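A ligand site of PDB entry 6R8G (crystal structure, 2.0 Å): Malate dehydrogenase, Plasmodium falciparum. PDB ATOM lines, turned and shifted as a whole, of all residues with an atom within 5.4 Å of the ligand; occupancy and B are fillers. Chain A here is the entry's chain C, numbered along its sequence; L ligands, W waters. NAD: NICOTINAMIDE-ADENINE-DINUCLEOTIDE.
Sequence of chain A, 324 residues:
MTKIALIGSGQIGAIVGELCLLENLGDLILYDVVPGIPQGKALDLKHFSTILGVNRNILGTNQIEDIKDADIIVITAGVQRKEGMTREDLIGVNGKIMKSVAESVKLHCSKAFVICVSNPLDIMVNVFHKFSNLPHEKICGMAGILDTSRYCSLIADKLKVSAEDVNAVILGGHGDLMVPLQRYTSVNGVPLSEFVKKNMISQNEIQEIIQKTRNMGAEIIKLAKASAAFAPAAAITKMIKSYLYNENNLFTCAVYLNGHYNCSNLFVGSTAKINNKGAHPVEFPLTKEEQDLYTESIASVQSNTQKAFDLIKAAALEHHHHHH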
ATOM      1  N   ILE A   7     -17.066  -7.206  21.249  1.00  0.00           N
ATOM      2  CA  ILE A   7     -17.935  -8.120  22.030  1.00  0.00           C
ATOM      3  C   ILE A   7     -18.799  -8.867  21.026  1.00  0.00           C
ATOM      4  O   ILE A   7     -19.859  -8.362  20.646  1.00  0.00           O
ATOM      5  CB  ILE A   7     -18.774  -7.416  23.095  1.00  0.00           C
ATOM      6  CG1 ILE A   7     -17.986  -6.433  23.934  1.00  0.00           C
ATOM      7  CG2 ILE A   7     -19.466  -8.436  23.959  1.00  0.00           C
ATOM      8  CD1 ILE A   7     -16.865  -7.010  24.674  1.00  0.00           C
ATOM      9  N   GLY A   8     -18.304 -10.036  20.623  1.00  0.00           N
ATOM     10  CA  GLY A   8     -18.836 -10.779  19.480  1.00  0.00           C
ATOM     11  C   GLY A   8     -17.786 -10.826  18.397  1.00  0.00           C
ATOM     12  O   GLY A   8     -17.345  -9.729  17.907  1.00  0.00           O
ATOM     13  N   SER A   9     -17.348 -12.031  18.081  1.00  0.00           N
ATOM     14  CA  SER A   9     -16.287 -12.310  17.082  1.00  0.00           C
ATOM     15  C   SER A   9     -16.864 -13.066  15.889  1.00  0.00           C
ATOM     16  O   SER A   9     -16.132 -13.915  15.350  1.00  0.00           O
ATOM     17  CB  SER A   9     -15.112 -12.992  17.729  1.00  0.00           C
ATOM     18  OG  SER A   9     -14.560 -12.153  18.754  1.00  0.00           O
ATOM     19  N   GLY A  10     -18.101 -12.744  15.510  1.00  0.00           N
ATOM     20  CA  GLY A  10     -18.794 -13.270  14.308  1.00  0.00           C
ATOM     21  C   GLY A  10     -18.361 -12.554  13.064  1.00  0.00           C
ATOM     22  O   GLY A  10     -17.291 -11.897  13.068  1.00  0.00           O
ATOM     23  N   GLN A  11     -19.200 -12.580  12.048  1.00  0.00           N
ATOM     24  CA  GLN A  11     -18.862 -12.044  10.716  1.00  0.00           C
ATOM     25  C   GLN A  11     -18.620 -10.542  10.856  1.00  0.00           C
ATOM     26  O   GLN A  11     -17.611 -10.037  10.326  1.00  0.00           O
ATOM     27  CB  GLN A  11     -20.043 -12.388   9.832  1.00  0.00           C
ATOM     28  CG  GLN A  11     -19.790 -12.072   8.379  1.00  0.00           C
ATOM     29  CD  GLN A  11     -18.873 -13.030   7.646  1.00  0.00           C
ATOM     30  OE1 GLN A  11     -18.684 -12.960   6.433  1.00  0.00           O
ATOM     31  NE2 GLN A  11     -18.395 -14.008   8.403  1.00  0.00           N
ATOM     32  N   ILE A  12     -19.529  -9.826  11.532  1.00  0.00           N
ATOM     33  CA  ILE A  12     -19.400  -8.342  11.599  1.00  0.00           C
ATOM     34  C   ILE A  12     -18.194  -8.000  12.484  1.00  0.00           C
ATOM     35  O   ILE A  12     -17.396  -7.099  12.130  1.00  0.00           O
ATOM     36  CB  ILE A  12     -20.693  -7.620  11.969  1.00  0.00           C
ATOM     37  CG1 ILE A  12     -21.670  -7.659  10.787  1.00  0.00           C
ATOM     38  CG2 ILE A  12     -20.396  -6.185  12.347  1.00  0.00           C
ATOM     39  CD1 ILE A  12     -23.057  -7.171  11.116  1.00  0.00           C
ATOM     40  N   GLY A  13     -18.052  -8.664  13.606  1.00  0.00           N
ATOM     41  CA  GLY A  13     -16.992  -8.308  14.563  1.00  0.00           C
ATOM     42  C   GLY A  13     -15.627  -8.504  13.949  1.00  0.00           C
ATOM     43  O   GLY A  13     -14.741  -7.645  14.151  1.00  0.00           O
ATOM     44  N   TYR A  31     -13.463 -10.726  21.590  1.00  0.00           N
ATOM     45  CA  TYR A  31     -14.123 -11.481  22.659  1.00  0.00           C
ATOM     46  C   TYR A  31     -15.316 -12.228  22.092  1.00  0.00           C
ATOM     47  O   TYR A  31     -16.032 -11.704  21.201  1.00  0.00           O
ATOM     48  CB  TYR A  31     -14.516 -10.578  23.830  1.00  0.00           C
ATOM     49  CG  TYR A  31     -15.413 -11.300  24.787  1.00  0.00           C
ATOM     50  CD1 TYR A  31     -14.905 -12.184  25.741  1.00  0.00           C
ATOM     51  CD2 TYR A  31     -16.770 -11.161  24.689  1.00  0.00           C
ATOM     52  CE1 TYR A  31     -15.745 -12.890  26.584  1.00  0.00           C
ATOM     53  CE2 TYR A  31     -17.626 -11.854  25.530  1.00  0.00           C
ATOM     54  CZ  TYR A  31     -17.111 -12.717  26.474  1.00  0.00           C
ATOM     55  OH  TYR A  31     -17.983 -13.309  27.311  1.00  0.00           O
ATOM     56  N   ASP A  32     -15.542 -13.433  22.580  1.00  0.00           N
ATOM     57  CA  ASP A  32     -16.777 -14.214  22.286  1.00  0.00           C
ATOM     58  C   ASP A  32     -17.000 -15.194  23.432  1.00  0.00           C
ATOM     59  O   ASP A  32     -16.029 -15.556  24.106  1.00  0.00           O
ATOM     60  CB  ASP A  32     -16.706 -14.889  20.928  1.00  0.00           C
ATOM     61  CG  ASP A  32     -18.052 -15.094  20.286  1.00  0.00           C
ATOM     62  OD1 ASP A  32     -18.768 -16.045  20.692  1.00  0.00           O
ATOM     63  OD2 ASP A  32     -18.360 -14.360  19.350  1.00  0.00           O
ATOM     64  N   VAL A  33     -18.228 -15.685  23.596  1.00  0.00           N
ATOM     65  CA  VAL A  33     -18.528 -16.741  24.606  1.00  0.00           C
ATOM     66  C   VAL A  33     -18.085 -18.094  24.073  1.00  0.00           C
ATOM     67  O   VAL A  33     -17.870 -18.932  24.912  1.00  0.00           O
ATOM     68  CB  VAL A  33     -20.010 -16.799  25.018  1.00  0.00           C
ATOM     69  CG1 VAL A  33     -20.347 -15.617  25.923  1.00  0.00           C
ATOM     70  CG2 VAL A  33     -20.929 -16.962  23.787  1.00  0.00           C
ATOM     71  N   VAL A  34     -18.052 -18.320  22.769  1.00  0.00           N
ATOM     72  CA  VAL A  34     -17.775 -19.643  22.170  1.00  0.00           C
ATOM     73  C   VAL A  34     -16.278 -19.923  22.197  1.00  0.00           C
ATOM     74  O   VAL A  34     -15.497 -19.200  21.591  1.00  0.00           O
ATOM     75  CB  VAL A  34     -18.306 -19.810  20.739  1.00  0.00           C
ATOM     76  CG1 VAL A  34     -18.048 -21.233  20.215  1.00  0.00           C
ATOM     77  CG2 VAL A  34     -19.786 -19.446  20.639  1.00  0.00           C
ATOM     78  N   ILE A  37     -13.364 -19.551  18.999  1.00  0.00           N
ATOM     79  CA  ILE A  37     -13.725 -18.685  17.839  1.00  0.00           C
ATOM     80  C   ILE A  37     -12.819 -17.462  17.814  1.00  0.00           C
ATOM     81  O   ILE A  37     -12.169 -17.189  16.814  1.00  0.00           O
ATOM     82  CB  ILE A  37     -15.228 -18.376  17.744  1.00  0.00           C
ATOM     83  CG1 ILE A  37     -15.911 -19.671  17.258  1.00  0.00           C
ATOM     84  CG2 ILE A  37     -15.530 -17.201  16.793  1.00  0.00           C
ATOM     85  CD1 ILE A  37     -17.407 -19.602  17.227  1.00  0.00           C
ATOM     86  N   THR A  76     -21.690  -6.921  18.927  1.00  0.00           N
ATOM     87  CA  THR A  76     -22.419  -7.712  17.932  1.00  0.00           C
ATOM     88  C   THR A  76     -22.973  -8.991  18.560  1.00  0.00           C
ATOM     89  O   THR A  76     -23.543  -9.791  17.814  1.00  0.00           O
ATOM     90  CB  THR A  76     -21.531  -8.035  16.725  1.00  0.00           C
ATOM     91  OG1 THR A  76     -20.334  -8.724  17.167  1.00  0.00           O
ATOM     92  CG2 THR A  76     -21.335  -6.790  15.932  1.00  0.00           C
ATOM     93  N   ALA A  77     -22.773  -9.187  19.850  1.00  0.00           N
ATOM     94  CA  ALA A  77     -23.156 -10.391  20.597  1.00  0.00           C
ATOM     95  C   ALA A  77     -24.659 -10.596  20.412  1.00  0.00           C
ATOM     96  O   ALA A  77     -25.474  -9.681  20.612  1.00  0.00           O
ATOM     97  CB  ALA A  77     -22.758 -10.264  22.049  1.00  0.00           C
ATOM     98  N   GLY A  78     -25.024 -11.814  20.064  1.00  0.00           N
ATOM     99  CA  GLY A  78     -26.436 -12.215  19.997  1.00  0.00           C
ATOM    100  C   GLY A  78     -26.572 -13.374  19.059  1.00  0.00           C
ATOM    101  O   GLY A  78     -25.484 -13.924  18.654  1.00  0.00           O
ATOM    102  N   VAL A  79     -27.790 -13.764  18.727  1.00  0.00           N
ATOM    103  CA  VAL A  79     -27.997 -14.924  17.808  1.00  0.00           C
ATOM    104  C   VAL A  79     -28.842 -14.423  16.631  1.00  0.00           C
ATOM    105  O   VAL A  79     -29.426 -13.323  16.746  1.00  0.00           O
ATOM    106  CB  VAL A  79     -28.676 -16.100  18.548  1.00  0.00           C
ATOM    107  CG1 VAL A  79     -27.793 -16.610  19.691  1.00  0.00           C
ATOM    108  CG2 VAL A  79     -30.056 -15.701  19.031  1.00  0.00           C
ATOM    109  N   GLN A  80     -28.880 -15.206  15.552  1.00  0.00           N
ATOM    110  CA  GLN A  80     -29.867 -15.020  14.442  1.00  0.00           C
ATOM    111  C   GLN A  80     -31.094 -15.859  14.789  1.00  0.00           C
ATOM    112  O   GLN A  80     -30.948 -16.910  15.429  1.00  0.00           O
ATOM    113  CB  GLN A  80     -29.329 -15.432  13.056  1.00  0.00           C
ATOM    114  CG  GLN A  80     -28.027 -14.765  12.617  1.00  0.00           C
ATOM    115  CD  GLN A  80     -28.074 -13.257  12.448  1.00  0.00           C
ATOM    116  OE1 GLN A  80     -28.721 -12.552  13.198  1.00  0.00           O
ATOM    117  NE2 GLN A  80     -27.338 -12.713  11.505  1.00  0.00           N
ATOM    118  N   ASN A  94     -31.507 -12.020  22.777  1.00  0.00           N
ATOM    119  CA  ASN A  94     -30.507 -10.941  22.501  1.00  0.00           C
ATOM    120  C   ASN A  94     -30.580  -9.883  23.615  1.00  0.00           C
ATOM    121  O   ASN A  94     -29.538  -9.269  23.936  1.00  0.00           O
ATOM    122  CB  ASN A  94     -30.652 -10.338  21.101  1.00  0.00           C
ATOM    123  CG  ASN A  94     -30.042 -11.262  20.076  1.00  0.00           C
ATOM    124  OD1 ASN A  94     -29.606 -12.326  20.392  1.00  0.00           O
ATOM    125  ND2 ASN A  94     -29.989 -10.853  18.826  1.00  0.00           N
ATOM    126  N   ILE A  97     -28.669 -11.198  26.548  1.00  0.00           N
ATOM    127  CA  ILE A  97     -27.238 -11.098  26.194  1.00  0.00           C
ATOM    128  C   ILE A  97     -26.789  -9.647  26.361  1.00  0.00           C
ATOM    129  O   ILE A  97     -25.783  -9.406  26.973  1.00  0.00           O
ATOM    130  CB  ILE A  97     -27.001 -11.697  24.804  1.00  0.00           C
ATOM    131  CG1 ILE A  97     -27.090 -13.231  24.908  1.00  0.00           C
ATOM    132  CG2 ILE A  97     -25.691 -11.214  24.195  1.00  0.00           C
ATOM    133  CD1 ILE A  97     -27.321 -13.910  23.561  1.00  0.00           C
ATOM    134  N   VAL A 101     -23.860  -8.137  28.751  1.00  0.00           N
ATOM    135  CA  VAL A 101     -22.753  -7.311  28.209  1.00  0.00           C
ATOM    136  C   VAL A 101     -22.736  -5.957  28.929  1.00  0.00           C
ATOM    137  O   VAL A 101     -21.667  -5.521  29.364  1.00  0.00           O
ATOM    138  CB  VAL A 101     -22.883  -7.181  26.673  1.00  0.00           C
ATOM    139  CG1 VAL A 101     -21.828  -6.231  26.143  1.00  0.00           C
ATOM    140  CG2 VAL A 101     -22.738  -8.569  26.027  1.00  0.00           C
ATOM    141  N   VAL A 117     -24.702  -2.959  18.035  1.00  0.00           N
ATOM    142  CA  VAL A 117     -24.992  -3.379  16.643  1.00  0.00           C
ATOM    143  C   VAL A 117     -26.039  -4.497  16.622  1.00  0.00           C
ATOM    144  O   VAL A 117     -26.832  -4.493  15.654  1.00  0.00           O
ATOM    145  CB  VAL A 117     -23.703  -3.758  15.883  1.00  0.00           C
ATOM    146  CG1 VAL A 117     -23.990  -3.978  14.396  1.00  0.00           C
ATOM    147  CG2 VAL A 117     -22.630  -2.705  16.083  1.00  0.00           C
ATOM    148  N   SER A 118     -26.170  -5.281  17.677  1.00  0.00           N
ATOM    149  CA  SER A 118     -27.139  -6.412  17.782  1.00  0.00           C
ATOM    150  C   SER A 118     -28.578  -6.039  17.447  1.00  0.00           C
ATOM    151  O   SER A 118     -29.060  -4.953  17.903  1.00  0.00           O
ATOM    152  CB  SER A 118     -27.080  -6.979  19.161  1.00  0.00           C
ATOM    153  OG  SER A 118     -25.729  -7.303  19.480  1.00  0.00           O
ATOM    154  N   ASN A 119     -29.296  -6.970  16.833  1.00  0.00           N
ATOM    155  CA  ASN A 119     -30.677  -6.715  16.385  1.00  0.00           C
ATOM    156  C   ASN A 119     -31.656  -7.212  17.435  1.00  0.00           C
ATOM    157  O   ASN A 119     -31.369  -8.059  18.276  1.00  0.00           O
ATOM    158  CB  ASN A 119     -30.944  -7.234  14.962  1.00  0.00           C
ATOM    159  CG  ASN A 119     -30.664  -6.143  13.933  1.00  0.00           C
ATOM    160  OD1 ASN A 119     -30.974  -4.946  14.154  1.00  0.00           O
ATOM    161  ND2 ASN A 119     -30.037  -6.516  12.830  1.00  0.00           N
ATOM    162  N   LEU A 121     -31.834  -3.413  16.432  1.00  0.00           N
ATOM    163  CA  LEU A 121     -30.886  -2.369  16.892  1.00  0.00           C
ATOM    164  C   LEU A 121     -31.553  -1.318  17.780  1.00  0.00           C
ATOM    165  O   LEU A 121     -30.984  -1.020  18.805  1.00  0.00           O
ATOM    166  CB  LEU A 121     -30.223  -1.575  15.754  1.00  0.00           C
ATOM    167  CG  LEU A 121     -29.308  -0.522  16.411  1.00  0.00           C
ATOM    168  CD1 LEU A 121     -27.903  -0.967  16.333  1.00  0.00           C
ATOM    169  CD2 LEU A 121     -29.505   0.903  15.919  1.00  0.00           C
ATOM    170  N   MET A 142     -25.253   1.769  15.687  1.00  0.00           N
ATOM    171  CA  MET A 142     -24.984   1.939  14.252  1.00  0.00           C
ATOM    172  C   MET A 142     -26.223   1.423  13.550  1.00  0.00           C
ATOM    173  O   MET A 142     -26.536   0.245  13.768  1.00  0.00           O
ATOM    174  CB  MET A 142     -23.762   1.114  13.827  1.00  0.00           C
ATOM    175  CG  MET A 142     -23.353   1.318  12.372  1.00  0.00           C
ATOM    176  SD  MET A 142     -24.428   0.489  11.191  1.00  0.00           S
ATOM    177  CE  MET A 142     -24.339  -1.215  11.741  1.00  0.00           C
ATOM    178  N   ALA A 143     -26.889   2.294  12.778  1.00  0.00           N
ATOM    179  CA  ALA A 143     -27.942   1.930  11.808  1.00  0.00           C
ATOM    180  C   ALA A 143     -27.994   2.928  10.636  1.00  0.00           C
ATOM    181  O   ALA A 143     -27.848   2.456   9.449  1.00  0.00           O
ATOM    182  CB  ALA A 143     -29.277   1.812  12.523  1.00  0.00           C
ATOM    183  N   LEU A 146     -25.998   3.093   7.281  1.00  0.00           N
ATOM    184  CA  LEU A 146     -26.248   2.048   6.254  1.00  0.00           C
ATOM    185  C   LEU A 146     -27.358   2.532   5.319  1.00  0.00           C
ATOM    186  O   LEU A 146     -27.197   2.514   4.130  1.00  0.00           O
ATOM    187  CB  LEU A 146     -26.702   0.769   6.935  1.00  0.00           C
ATOM    188  CG  LEU A 146     -25.726  -0.375   7.109  1.00  0.00           C
ATOM    189  CD1 LEU A 146     -26.553  -1.612   7.459  1.00  0.00           C
ATOM    190  CD2 LEU A 146     -24.865  -0.600   5.861  1.00  0.00           C
ATOM    191  N   HIS A 174     -34.491   1.267  10.683  1.00  0.00           N
ATOM    192  CA  HIS A 174     -34.554   0.499   9.395  1.00  0.00           C
ATOM    193  C   HIS A 174     -36.027   0.324   8.980  1.00  0.00           C
ATOM    194  O   HIS A 174     -36.898   0.400   9.839  1.00  0.00           O
ATOM    195  CB  HIS A 174     -33.821  -0.851   9.513  1.00  0.00           C
ATOM    196  CG  HIS A 174     -32.335  -0.749   9.652  1.00  0.00           C
ATOM    197  ND1 HIS A 174     -31.575   0.250   9.035  1.00  0.00           N
ATOM    198  CD2 HIS A 174     -31.457  -1.531  10.336  1.00  0.00           C
ATOM    199  CE1 HIS A 174     -30.300   0.078   9.327  1.00  0.00           C
ATOM    200  NE2 HIS A 174     -30.199  -1.014  10.127  1.00  0.00           N
ATOM    201  N   SER A 227     -27.048 -11.809   6.460  1.00  0.00           N
ATOM    202  CA  SER A 227     -27.275 -10.353   6.582  1.00  0.00           C
ATOM    203  C   SER A 227     -25.980  -9.657   6.183  1.00  0.00           C
ATOM    204  O   SER A 227     -24.904 -10.318   6.119  1.00  0.00           O
ATOM    205  CB  SER A 227     -27.768  -9.927   7.926  1.00  0.00           C
ATOM    206  OG  SER A 227     -27.207 -10.732   8.908  1.00  0.00           O
ATOM    207  N   ALA A 228     -26.131  -8.410   5.762  1.00  0.00           N
ATOM    208  CA  ALA A 228     -25.019  -7.560   5.346  1.00  0.00           C
ATOM    209  C   ALA A 228     -23.917  -7.624   6.417  1.00  0.00           C
ATOM    210  O   ALA A 228     -24.252  -7.679   7.608  1.00  0.00           O
ATOM    211  CB  ALA A 228     -25.575  -6.180   5.110  1.00  0.00           C
ATOM    212  N   ALA A 229     -22.642  -7.616   6.011  1.00  0.00           N
ATOM    213  CA  ALA A 229     -21.524  -7.647   6.979  1.00  0.00           C
ATOM    214  C   ALA A 229     -20.471  -6.565   6.634  1.00  0.00           C
ATOM    215  O   ALA A 229     -20.055  -5.851   7.548  1.00  0.00           O
ATOM    216  CB  ALA A 229     -20.953  -9.057   7.006  1.00  0.00           C
ATOM    217  N   PRO A 232     -22.024  -2.716   7.223  1.00  0.00           N
ATOM    218  CA  PRO A 232     -22.136  -2.483   8.667  1.00  0.00           C
ATOM    219  C   PRO A 232     -20.774  -2.271   9.337  1.00  0.00           C
ATOM    220  O   PRO A 232     -20.634  -1.355  10.147  1.00  0.00           O
ATOM    221  CB  PRO A 232     -22.798  -3.749   9.190  1.00  0.00           C
ATOM    222  CG  PRO A 232     -23.572  -4.288   7.993  1.00  0.00           C
ATOM    223  CD  PRO A 232     -22.772  -3.911   6.781  1.00  0.00           C
HETATM  224  PA  NAD L   1     -22.849 -13.630  14.046  1.00  0.00           P
HETATM  225  O1A NAD L   1     -21.912 -13.805  12.852  1.00  0.00           O
HETATM  226  O2A NAD L   1     -23.891 -14.608  14.501  1.00  0.00           O
HETATM  227  O5B NAD L   1     -21.957 -13.201  15.323  1.00  0.00           O
HETATM  228  C5B NAD L   1     -22.457 -12.896  16.631  1.00  0.00           C
HETATM  229  C4B NAD L   1     -21.431 -13.407  17.602  1.00  0.00           C
HETATM  230  O4B NAD L   1     -21.889 -13.108  18.947  1.00  0.00           O
HETATM  231  C3B NAD L   1     -21.181 -14.936  17.531  1.00  0.00           C
HETATM  232  O3B NAD L   1     -19.800 -15.272  17.354  1.00  0.00           O
HETATM  233  C2B NAD L   1     -21.736 -15.458  18.862  1.00  0.00           C
HETATM  234  O2B NAD L   1     -20.994 -16.574  19.352  1.00  0.00           O
HETATM  235  C1B NAD L   1     -21.559 -14.216  19.743  1.00  0.00           C
HETATM  236  N9A NAD L   1     -22.317 -14.208  20.998  1.00  0.00           N
HETATM  237  C8A NAD L   1     -23.510 -14.855  21.267  1.00  0.00           C
HETATM  238  N7A NAD L   1     -23.860 -14.765  22.533  1.00  0.00           N
HETATM  239  C5A NAD L   1     -22.853 -13.983  23.118  1.00  0.00           C
HETATM  240  C6A NAD L   1     -22.654 -13.554  24.443  1.00  0.00           C
HETATM  241  N6A NAD L   1     -23.480 -13.887  25.450  1.00  0.00           N
HETATM  242  N1A NAD L   1     -21.566 -12.777  24.704  1.00  0.00           N
HETATM  243  C2A NAD L   1     -20.717 -12.542  23.680  1.00  0.00           C
HETATM  244  N3A NAD L   1     -20.734 -12.969  22.411  1.00  0.00           N
HETATM  245  C4A NAD L   1     -21.861 -13.678  22.191  1.00  0.00           C
HETATM  246  O3  NAD L   1     -23.572 -12.240  13.624  1.00  0.00           O
HETATM  247  PN  NAD L   1     -23.064 -11.033  12.668  1.00  0.00           P
HETATM  248  O1N NAD L   1     -21.667 -10.580  13.077  1.00  0.00           O
HETATM  249  O2N NAD L   1     -23.228 -11.379  11.229  1.00  0.00           O
HETATM  250  O5D NAD L   1     -24.190  -9.929  13.121  1.00  0.00           O
HETATM  251  C5D NAD L   1     -24.237  -9.540  14.513  1.00  0.00           C
HETATM  252  C4D NAD L   1     -25.479  -8.753  14.835  1.00  0.00           C
HETATM  253  O4D NAD L   1     -25.518  -7.545  14.038  1.00  0.00           O
HETATM  254  C3D NAD L   1     -26.826  -9.488  14.575  1.00  0.00           C
HETATM  255  O3D NAD L   1     -27.684  -9.192  15.679  1.00  0.00           O
HETATM  256  C2D NAD L   1     -27.347  -8.872  13.253  1.00  0.00           C
HETATM  257  O2D NAD L   1     -28.766  -8.954  13.156  1.00  0.00           O
HETATM  258  C1D NAD L   1     -26.854  -7.429  13.444  1.00  0.00           C
HETATM  259  N1N NAD L   1     -26.844  -6.548  12.231  1.00  0.00           N
HETATM  260  C2N NAD L   1     -27.162  -5.214  12.422  1.00  0.00           C
HETATM  261  C3N NAD L   1     -27.145  -4.269  11.372  1.00  0.00           C
HETATM  262  C7N NAD L   1     -27.481  -2.834  11.757  1.00  0.00           C
HETATM  263  O7N NAD L   1     -27.817  -2.032  10.883  1.00  0.00           O
HETATM  264  N7N NAD L   1     -27.422  -2.492  13.044  1.00  0.00           N
HETATM  265  C4N NAD L   1     -26.895  -4.748  10.076  1.00  0.00           C
HETATM  266  C5N NAD L   1     -26.768  -6.151   9.852  1.00  0.00           C
HETATM  267  C6N NAD L   1     -26.627  -7.016  10.947  1.00  0.00           C
HETATM  268  O   HOH W   1     -20.428 -12.228  27.421  1.00  0.00           O
HETATM  269  O   HOH W   2     -19.930 -10.403  15.196  1.00  0.00           O
HETATM  270  O   HOH W   3     -20.616 -16.173  12.566  1.00  0.00           O
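OD2 of Asp 32 lies within hydrogen-bond range of O3B of the ligand (2.6 Å).
A ring nitrogen (NE2) of His 174 sits at hydrogen-bond distance from an oxygen (O7N) of the ligand, at 2.7 Å.
The backbone NH of Ile 12 lies within hydrogen-bond range of an oxygen (O1N) of the ligand (2.7 Å).
The backbone NH (N) of Asn 119 is in hydrogen-bond range of an oxygen (O3D) of the ligand, at 3.0 Å.
An oxygen (O2D) of the ligand lies within hydrogen-bond range of the side-chain amide nitrogen of Asn 119 (2.8 Å).
The backbone carbonyl oxygen (O) of Met 142 sits at hydrogen-bond distance from a nitrogen (N7N) of the ligand, 3.0 Å away.
N of Gln 11 is in hydrogen-bond range of O1A of the ligand, 3.1 Å away.
The backbone carbonyl oxygen of Val 117 lies close to a nitrogen (N7N) of the ligand (3.3 Å).
Water W2 lies within hydrogen-bond range of the side-chain hydroxyl of Thr 76 (2.6 Å), an oxygen (O1N) of the ligand (2.7 Å), the backbone NH of Gly 10 (3.0 Å) and the backbone NH of Gly 13 (3.0 Å).
Water W1 bridges the side-chain hydroxyl of Tyr 31 (2.7 Å) and a nitrogen (N1A) of the ligand (3.0 Å).
The backbone NH (N) of Val 34 is in hydrogen-bond range of the side-chain carboxylate (OD1) of Asp 32, at 3.2 Å.
The side-chain amide oxygen of Asn 119 sits at hydrogen-bond distance from the backbone NH of Leu 121 (2.9 Å).
The backbone carbonyl oxygen (O) of Asn 119 lies within hydrogen-bond range of the side-chain amide nitrogen (ND2) of Asn 94 (3.2 Å).
O of Gly 8 is in hydrogen-bond range of OG1 of Thr 76 (3.2 Å).
The backbone carbonyl oxygen (O) of Ile 7 sits at hydrogen-bond distance from the backbone NH (N) of Thr 76.
O of Ala 77 is in hydrogen-bond range of OG of Ser 118, at 2.6 Å.
The backbone NH (N) of Ala 77 lies within hydrogen-bond range of the backbone carbonyl oxygen (O) of Ile 7 (3.1 Å).
O of Tyr 31 is in hydrogen-bond range of OG of Ser 9 (2.9 Å).
Merely in contact with the ligand: Gly 8, Ser 9, Gly 10, Tyr 31, Val 33, Val 34, Thr 76, Ala 77, Gly 78, Gln 80, Ile 97, Ser 118, Leu 121, Leu 146, Ala 228 and Pro 232.
Hydrophobic or aromatic side chains within 4 Å of the ligand: Ile 12, Tyr 31, Val 33, Val 34, Ala 77, Ile 97, Val 117, Leu 121, Met 142, Leu 146, His 174 and Pro 232.
Of the 32 residues printed, 23 come within 4 Å of the ligand.
The nearest printed residue that does not touch the ligand is Ala 143 (4.1 Å).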
